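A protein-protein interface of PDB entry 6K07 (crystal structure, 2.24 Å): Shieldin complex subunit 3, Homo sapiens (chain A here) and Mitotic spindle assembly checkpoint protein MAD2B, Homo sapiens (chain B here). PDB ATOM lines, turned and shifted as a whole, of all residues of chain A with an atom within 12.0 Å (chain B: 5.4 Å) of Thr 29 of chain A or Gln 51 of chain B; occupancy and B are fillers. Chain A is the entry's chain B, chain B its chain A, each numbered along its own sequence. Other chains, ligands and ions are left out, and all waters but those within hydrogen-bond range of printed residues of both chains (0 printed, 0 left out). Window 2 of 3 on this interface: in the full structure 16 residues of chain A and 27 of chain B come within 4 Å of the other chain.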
ATOM      1  N   ILE A  16       8.716 -41.091 -12.866  1.00  0.00           N
ATOM      2  CA  ILE A  16       9.377 -40.008 -12.149  1.00  0.00           C
ATOM      3  C   ILE A  16       9.672 -40.495 -10.740  1.00  0.00           C
ATOM      4  O   ILE A  16       8.749 -40.681  -9.934  1.00  0.00           O
ATOM      5  CB  ILE A  16       8.541 -38.728 -12.125  1.00  0.00           C
ATOM      6  CG1 ILE A  16       8.187 -38.297 -13.546  1.00  0.00           C
ATOM      7  CG2 ILE A  16       9.294 -37.587 -11.414  1.00  0.00           C
ATOM      8  CD1 ILE A  16       7.526 -36.933 -13.595  1.00  0.00           C
ATOM      9  N   GLU A  18      11.027 -40.150  -6.883  1.00  0.00           N
ATOM     10  CA  GLU A  18      10.788 -39.079  -5.923  1.00  0.00           C
ATOM     11  C   GLU A  18      12.039 -38.252  -5.675  1.00  0.00           C
ATOM     12  O   GLU A  18      11.933 -37.088  -5.266  1.00  0.00           O
ATOM     13  CB  GLU A  18      10.245 -39.642  -4.603  1.00  0.00           C
ATOM     14  CG  GLU A  18       9.977 -38.568  -3.536  1.00  0.00           C
ATOM     15  CD  GLU A  18       8.508 -38.500  -3.118  1.00  0.00           C
ATOM     16  OE1 GLU A  18       8.073 -37.426  -2.647  1.00  0.00           O
ATOM     17  OE2 GLU A  18       7.787 -39.510  -3.260  1.00  0.00           O
ATOM     18  N   GLU A  19      13.220 -38.813  -5.922  1.00  0.00           N
ATOM     19  CA  GLU A  19      14.407 -37.975  -5.913  1.00  0.00           C
ATOM     20  C   GLU A  19      14.334 -36.966  -7.047  1.00  0.00           C
ATOM     21  O   GLU A  19      14.547 -35.766  -6.843  1.00  0.00           O
ATOM     22  CB  GLU A  19      15.670 -38.833  -6.004  1.00  0.00           C
ATOM     23  CG  GLU A  19      15.828 -39.599  -7.303  1.00  0.00           C
ATOM     24  CD  GLU A  19      16.890 -40.669  -7.219  1.00  0.00           C
ATOM     25  OE1 GLU A  19      18.033 -40.419  -7.669  1.00  0.00           O
ATOM     26  OE2 GLU A  19      16.571 -41.766  -6.714  1.00  0.00           O
ATOM     27  N   ALA A  20      13.974 -37.434  -8.245  1.00  0.00           N
ATOM     28  CA  ALA A  20      13.785 -36.533  -9.373  1.00  0.00           C
ATOM     29  C   ALA A  20      12.719 -35.493  -9.076  1.00  0.00           C
ATOM     30  O   ALA A  20      12.842 -34.340  -9.500  1.00  0.00           O
ATOM     31  CB  ALA A  20      13.413 -37.335 -10.619  1.00  0.00           C
ATOM     32  N   ALA A  21      11.668 -35.881  -8.349  1.00  0.00           N
ATOM     33  CA  ALA A  21      10.641 -34.913  -7.977  1.00  0.00           C
ATOM     34  C   ALA A  21      11.172 -33.926  -6.945  1.00  0.00           C
ATOM     35  O   ALA A  21      10.844 -32.735  -6.991  1.00  0.00           O
ATOM     36  CB  ALA A  21       9.406 -35.635  -7.447  1.00  0.00           C
ATOM     37  N   GLU A  22      12.007 -34.399  -6.009  1.00  0.00           N
ATOM     38  CA  GLU A  22      12.641 -33.474  -5.074  1.00  0.00           C
ATOM     39  C   GLU A  22      13.566 -32.518  -5.807  1.00  0.00           C
ATOM     40  O   GLU A  22      13.651 -31.335  -5.462  1.00  0.00           O
ATOM     41  CB  GLU A  22      13.401 -34.241  -3.999  1.00  0.00           C
ATOM     42  N   ASP A  23      14.263 -33.007  -6.831  1.00  0.00           N
ATOM     43  CA  ASP A  23      15.096 -32.118  -7.631  1.00  0.00           C
ATOM     44  C   ASP A  23      14.241 -31.103  -8.355  1.00  0.00           C
ATOM     45  O   ASP A  23      14.559 -29.914  -8.376  1.00  0.00           O
ATOM     46  CB  ASP A  23      15.926 -32.915  -8.630  1.00  0.00           C
ATOM     47  CG  ASP A  23      17.164 -33.537  -7.997  1.00  0.00           C
ATOM     48  OD1 ASP A  23      17.259 -33.546  -6.746  1.00  0.00           O
ATOM     49  OD2 ASP A  23      18.023 -34.041  -8.759  1.00  0.00           O
ATOM     50  N   VAL A  24      13.135 -31.544  -8.945  1.00  0.00           N
ATOM     51  CA  VAL A  24      12.263 -30.582  -9.607  1.00  0.00           C
ATOM     52  C   VAL A  24      11.784 -29.550  -8.600  1.00  0.00           C
ATOM     53  O   VAL A  24      11.898 -28.338  -8.821  1.00  0.00           O
ATOM     54  CB  VAL A  24      11.085 -31.288 -10.304  1.00  0.00           C
ATOM     55  CG1 VAL A  24      10.099 -30.272 -10.780  1.00  0.00           C
ATOM     56  CG2 VAL A  24      11.579 -32.139 -11.468  1.00  0.00           C
ATOM     57  N   LYS A  25      11.261 -30.018  -7.468  1.00  0.00           N
ATOM     58  CA  LYS A  25      10.798 -29.098  -6.440  1.00  0.00           C
ATOM     59  C   LYS A  25      11.916 -28.164  -6.024  1.00  0.00           C
ATOM     60  O   LYS A  25      11.703 -26.966  -5.829  1.00  0.00           O
ATOM     61  CB  LYS A  25      10.265 -29.890  -5.249  1.00  0.00           C
ATOM     62  CG  LYS A  25      10.199 -29.120  -3.971  1.00  0.00           C
ATOM     63  CD  LYS A  25       9.180 -27.994  -4.042  1.00  0.00           C
ATOM     64  CE  LYS A  25       9.566 -26.865  -3.072  1.00  0.00           C
ATOM     65  NZ  LYS A  25       8.407 -26.045  -2.572  1.00  0.00           N
ATOM     66  N   GLN A  26      13.131 -28.681  -5.975  1.00  0.00           N
ATOM     67  CA  GLN A  26      14.258 -27.936  -5.431  1.00  0.00           C
ATOM     68  C   GLN A  26      14.869 -26.947  -6.421  1.00  0.00           C
ATOM     69  O   GLN A  26      15.358 -25.892  -6.005  1.00  0.00           O
ATOM     70  CB  GLN A  26      15.332 -28.917  -4.973  1.00  0.00           C
ATOM     71  CG  GLN A  26      16.610 -28.281  -4.476  1.00  0.00           C
ATOM     72  CD  GLN A  26      16.545 -27.939  -3.010  1.00  0.00           C
ATOM     73  OE1 GLN A  26      15.655 -27.212  -2.568  1.00  0.00           O
ATOM     74  NE2 GLN A  26      17.483 -28.476  -2.241  1.00  0.00           N
ATOM     75  N   TYR A  27      14.885 -27.260  -7.710  1.00  0.00           N
ATOM     76  CA  TYR A  27      15.681 -26.490  -8.660  1.00  0.00           C
ATOM     77  C   TYR A  27      14.892 -25.874  -9.803  1.00  0.00           C
ATOM     78  O   TYR A  27      15.342 -24.878 -10.375  1.00  0.00           O
ATOM     79  CB  TYR A  27      16.777 -27.369  -9.262  1.00  0.00           C
ATOM     80  CG  TYR A  27      17.810 -27.805  -8.275  1.00  0.00           C
ATOM     81  CD1 TYR A  27      18.681 -26.886  -7.696  1.00  0.00           C
ATOM     82  CD2 TYR A  27      17.926 -29.130  -7.924  1.00  0.00           C
ATOM     83  CE1 TYR A  27      19.646 -27.292  -6.789  1.00  0.00           C
ATOM     84  CE2 TYR A  27      18.890 -29.549  -7.027  1.00  0.00           C
ATOM     85  CZ  TYR A  27      19.744 -28.635  -6.462  1.00  0.00           C
ATOM     86  OH  TYR A  27      20.696 -29.080  -5.561  1.00  0.00           O
ATOM     87  N   LEU A  28      13.760 -26.457 -10.182  1.00  0.00           N
ATOM     88  CA  LEU A  28      12.953 -25.926 -11.268  1.00  0.00           C
ATOM     89  C   LEU A  28      11.665 -25.302 -10.763  1.00  0.00           C
ATOM     90  O   LEU A  28      10.737 -25.107 -11.541  1.00  0.00           O
ATOM     91  CB  LEU A  28      12.679 -27.025 -12.288  1.00  0.00           C
ATOM     92  CG  LEU A  28      13.981 -27.742 -12.676  1.00  0.00           C
ATOM     93  CD1 LEU A  28      13.707 -28.952 -13.578  1.00  0.00           C
ATOM     94  CD2 LEU A  28      14.972 -26.766 -13.326  1.00  0.00           C
ATOM     95  N   THR A  29      11.622 -24.958  -9.481  1.00  0.00           N
ATOM     96  CA  THR A  29      10.471 -24.411  -8.770  1.00  0.00           C
ATOM     97  C   THR A  29       9.247 -25.258  -9.026  1.00  0.00           C
ATOM     98  O   THR A  29       9.068 -26.278  -8.356  1.00  0.00           O
ATOM     99  CB  THR A  29      10.192 -22.955  -9.145  1.00  0.00           C
ATOM    100  OG1 THR A  29      11.436 -22.269  -9.354  1.00  0.00           O
ATOM    101  CG2 THR A  29       9.491 -22.274  -7.986  1.00  0.00           C
ATOM    102  N   GLY B  48       5.586 -32.578  -5.740  1.00  0.00           N
ATOM    103  CA  GLY B  48       6.670 -31.617  -5.778  1.00  0.00           C
ATOM    104  C   GLY B  48       7.062 -31.181  -7.168  1.00  0.00           C
ATOM    105  O   GLY B  48       7.638 -30.098  -7.328  1.00  0.00           O
ATOM    106  N   ILE B  49       6.754 -31.994  -8.183  1.00  0.00           N
ATOM    107  CA  ILE B  49       7.018 -31.591  -9.558  1.00  0.00           C
ATOM    108  C   ILE B  49       6.067 -30.515 -10.055  1.00  0.00           C
ATOM    109  O   ILE B  49       6.265 -30.002 -11.156  1.00  0.00           O
ATOM    110  CB  ILE B  49       6.948 -32.793 -10.524  1.00  0.00           C
ATOM    111  CG1 ILE B  49       5.488 -33.160 -10.786  1.00  0.00           C
ATOM    112  CG2 ILE B  49       7.718 -33.961  -9.965  1.00  0.00           C
ATOM    113  CD1 ILE B  49       5.267 -34.103 -11.963  1.00  0.00           C
ATOM    114  N   PHE B  50       5.041 -30.160  -9.293  1.00  0.00           N
ATOM    115  CA  PHE B  50       4.054 -29.197  -9.752  1.00  0.00           C
ATOM    116  C   PHE B  50       4.287 -27.842  -9.128  1.00  0.00           C
ATOM    117  O   PHE B  50       4.699 -27.731  -7.968  1.00  0.00           O
ATOM    118  CB  PHE B  50       2.630 -29.637  -9.422  1.00  0.00           C
ATOM    119  CG  PHE B  50       2.180 -30.754 -10.256  1.00  0.00           C
ATOM    120  CD1 PHE B  50       1.686 -30.524 -11.522  1.00  0.00           C
ATOM    121  CD2 PHE B  50       2.321 -32.051  -9.814  1.00  0.00           C
ATOM    122  CE1 PHE B  50       1.298 -31.592 -12.317  1.00  0.00           C
ATOM    123  CE2 PHE B  50       1.938 -33.113 -10.605  1.00  0.00           C
ATOM    124  CZ  PHE B  50       1.440 -32.890 -11.852  1.00  0.00           C
ATOM    125  N   GLN B  51       3.961 -26.816  -9.904  1.00  0.00           N
ATOM    126  CA  GLN B  51       3.961 -25.436  -9.457  1.00  0.00           C
ATOM    127  C   GLN B  51       2.571 -24.853  -9.636  1.00  0.00           C
ATOM    128  O   GLN B  51       1.935 -25.053 -10.670  1.00  0.00           O
ATOM    129  CB  GLN B  51       4.946 -24.613 -10.240  1.00  0.00           C
ATOM    130  CG  GLN B  51       4.987 -23.204  -9.797  1.00  0.00           C
ATOM    131  CD  GLN B  51       6.243 -22.567 -10.240  1.00  0.00           C
ATOM    132  OE1 GLN B  51       7.007 -22.073  -9.429  1.00  0.00           O
ATOM    133  NE2 GLN B  51       6.492 -22.591 -11.540  1.00  0.00           N
ATOM    134  N   LYS B  52       2.104 -24.130  -8.631  1.00  0.00           N
ATOM    135  CA  LYS B  52       0.821 -23.459  -8.740  1.00  0.00           C
ATOM    136  C   LYS B  52       0.980 -22.261  -9.659  1.00  0.00           C
ATOM    137  O   LYS B  52       1.964 -21.522  -9.565  1.00  0.00           O
ATOM    138  CB  LYS B  52       0.317 -23.023  -7.361  1.00  0.00           C
ATOM    139  CG  LYS B  52      -0.997 -22.292  -7.431  1.00  0.00           C
ATOM    140  CD  LYS B  52      -1.221 -21.426  -6.209  1.00  0.00           C
ATOM    141  CE  LYS B  52      -1.257 -22.244  -4.918  1.00  0.00           C
ATOM    142  NZ  LYS B  52      -2.488 -21.935  -4.113  1.00  0.00           N
ATOM    143  N   ARG B  53       0.020 -22.086 -10.565  1.00  0.00           N
ATOM    144  CA  ARG B  53       0.025 -21.010 -11.554  1.00  0.00           C
ATOM    145  C   ARG B  53      -1.427 -20.625 -11.840  1.00  0.00           C
ATOM    146  O   ARG B  53      -2.362 -21.267 -11.354  1.00  0.00           O
ATOM    147  CB  ARG B  53       0.751 -21.438 -12.847  1.00  0.00           C
ATOM    148  CG  ARG B  53       2.246 -21.790 -12.685  1.00  0.00           C
ATOM    149  CD  ARG B  53       3.122 -21.231 -13.807  1.00  0.00           C
ATOM    150  NE  ARG B  53       2.560 -20.009 -14.385  1.00  0.00           N
ATOM    151  CZ  ARG B  53       2.628 -19.671 -15.673  1.00  0.00           C
ATOM    152  NH1 ARG B  53       3.267 -20.459 -16.536  1.00  0.00           N
ATOM    153  NH2 ARG B  53       2.065 -18.536 -16.094  1.00  0.00           N
ATOM    154  N   VAL B  60      -4.269 -23.103 -11.335  1.00  0.00           N
ATOM    155  CA  VAL B  60      -3.960 -24.403 -11.932  1.00  0.00           C
ATOM    156  C   VAL B  60      -2.631 -24.900 -11.362  1.00  0.00           C
ATOM    157  O   VAL B  60      -1.971 -24.214 -10.572  1.00  0.00           O
ATOM    158  CB  VAL B  60      -3.907 -24.347 -13.472  1.00  0.00           C
ATOM    159  CG1 VAL B  60      -5.207 -23.825 -14.054  1.00  0.00           C
ATOM    160  CG2 VAL B  60      -2.755 -23.485 -13.936  1.00  0.00           C
ATOM    161  N   GLN B  61      -2.249 -26.125 -11.741  1.00  0.00           N
ATOM    162  CA  GLN B  61      -0.996 -26.739 -11.315  1.00  0.00           C
ATOM    163  C   GLN B  61      -0.291 -27.317 -12.529  1.00  0.00           C
ATOM    164  O   GLN B  61      -0.785 -28.271 -13.137  1.00  0.00           O
ATOM    165  CB  GLN B  61      -1.237 -27.838 -10.281  1.00  0.00           C
ATOM    166  CG  GLN B  61      -1.955 -27.362  -9.023  1.00  0.00           C
ATOM    167  CD  GLN B  61      -1.020 -26.795  -7.971  1.00  0.00           C
ATOM    168  OE1 GLN B  61       0.201 -26.882  -8.098  1.00  0.00           O
ATOM    169  NE2 GLN B  61      -1.593 -26.222  -6.917  1.00  0.00           N
ATOM    170  N   MET B  62       0.863 -26.760 -12.872  1.00  0.00           N
ATOM    171  CA  MET B  62       1.634 -27.230 -14.008  1.00  0.00           C
ATOM    172  C   MET B  62       2.868 -27.969 -13.507  1.00  0.00           C
ATOM    173  O   MET B  62       3.474 -27.564 -12.508  1.00  0.00           O
ATOM    174  CB  MET B  62       2.037 -26.054 -14.907  1.00  0.00           C
ATOM    175  CG  MET B  62       0.851 -25.203 -15.383  1.00  0.00           C
ATOM    176  SD  MET B  62      -0.142 -25.988 -16.668  1.00  0.00           S
ATOM    177  CE  MET B  62       1.057 -26.158 -18.012  1.00  0.00           C
ATOM    178  N   SER B  63       3.238 -29.053 -14.196  1.00  0.00           N
ATOM    179  CA  SER B  63       4.422 -29.802 -13.791  1.00  0.00           C
ATOM    180  C   SER B  63       5.665 -29.072 -14.288  1.00  0.00           C
ATOM    181  O   SER B  63       5.671 -28.495 -15.382  1.00  0.00           O
ATOM    182  CB  SER B  63       4.416 -31.232 -14.338  1.00  0.00           C
ATOM    183  OG  SER B  63       5.063 -31.288 -15.587  1.00  0.00           O
ATOM    184  N   CYS B  64       6.709 -29.066 -13.464  1.00  0.00           N
ATOM    185  CA  CYS B  64       7.996 -28.529 -13.867  1.00  0.00           C
ATOM    186  C   CYS B  64       8.957 -29.633 -14.286  1.00  0.00           C
ATOM    187  O   CYS B  64      10.156 -29.389 -14.395  1.00  0.00           O
ATOM    188  CB  CYS B  64       8.575 -27.671 -12.744  1.00  0.00           C
ATOM    189  SG  CYS B  64       7.761 -26.027 -12.676  1.00  0.00           S
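Of the printed residues of chain B, Thr 29 of chain A touches Gln 51.
Of chain A, only Lys 25 (3.4 Å) comes within 4 Å of Gly 48 of chain B.
No residue of chain A comes within 4 Å of Arg 53 of chain B.
No residue of chain A comes within 4 Å of Gln 61 of chain B.
Met 62 of chain B touches none of the printed residues of chain A.
Of the printed residues of chain B, Val 24 of chain A touches Ile 49 (3.6 Å) and Cys 64 (3.6 Å).
Of the printed residues of chain B, Leu 28 of chain A touches Cys 64.
Glu 22 of chain A touches none of the printed residues of chain B.
Glu 19 of chain A touches none of the printed residues of chain B.
The nearest residue of chain A that does not touch Gln 51 of chain B is Leu 28 of chain A (4.9 Å).
The nearest printed residue of chain B that does not touch Lys 25 of chain A is Ile 49 of chain B (5.0 Å).
The backbone carbonyl oxygen of Leu 28 of chain A lies within hydrogen-bond range of the side-chain sulfur of Cys 64 of chain B, at 3.3 Å.
Of the 11 printed residues of chain B, 4 touch a printed residue of chain A.
Printed residues of chain B that touch a printed residue of chain A: Gly 48, Ile 49, Gln 51 and Cys 64.
Hydrophobic or aromatic side chains of chain B that line the printed part of chain A: Ile 49.
Along chain B the printed residues that touch a printed residue of chain A span positions 48 to 64.
Hydrophobic or aromatic side chains of chain A within 4 Å of the printed part of chain B: Ile 16, Ala 21, Val 24 and Leu 28.
Among the printed residues, no Asp or Glu carboxylate lies within 4 Å of a Lys or Arg side-chain nitrogen of the other chain.
O of Ile 49 of chain B sits at hydrogen-bond distance from N of Cys 64 of chain B, at 2.5 Å.
The backbone carbonyl oxygen of Val 24 of chain A sits at hydrogen-bond distance from the backbone NH of Thr 29 of chain A (3.5 Å).
The backbone carbonyl oxygen (O) of Met 62 of chain B lies within hydrogen-bond range of the backbone NH (N) of Gln 51 of chain B (2.8 Å).
Among the printed residues, pairs that only touch across the chains: Ile 16 of chain A with Ile 49 of chain B, Ala 21 of chain A with Ile 49 of chain B, Val 24 of chain A with Ile 49 of chain B, Val 24 of chain A with Cys 64 of chain B, Lys 25 of chain A with Gly 48 of chain B and Thr 29 of chain A with Gln 51 of chain B.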
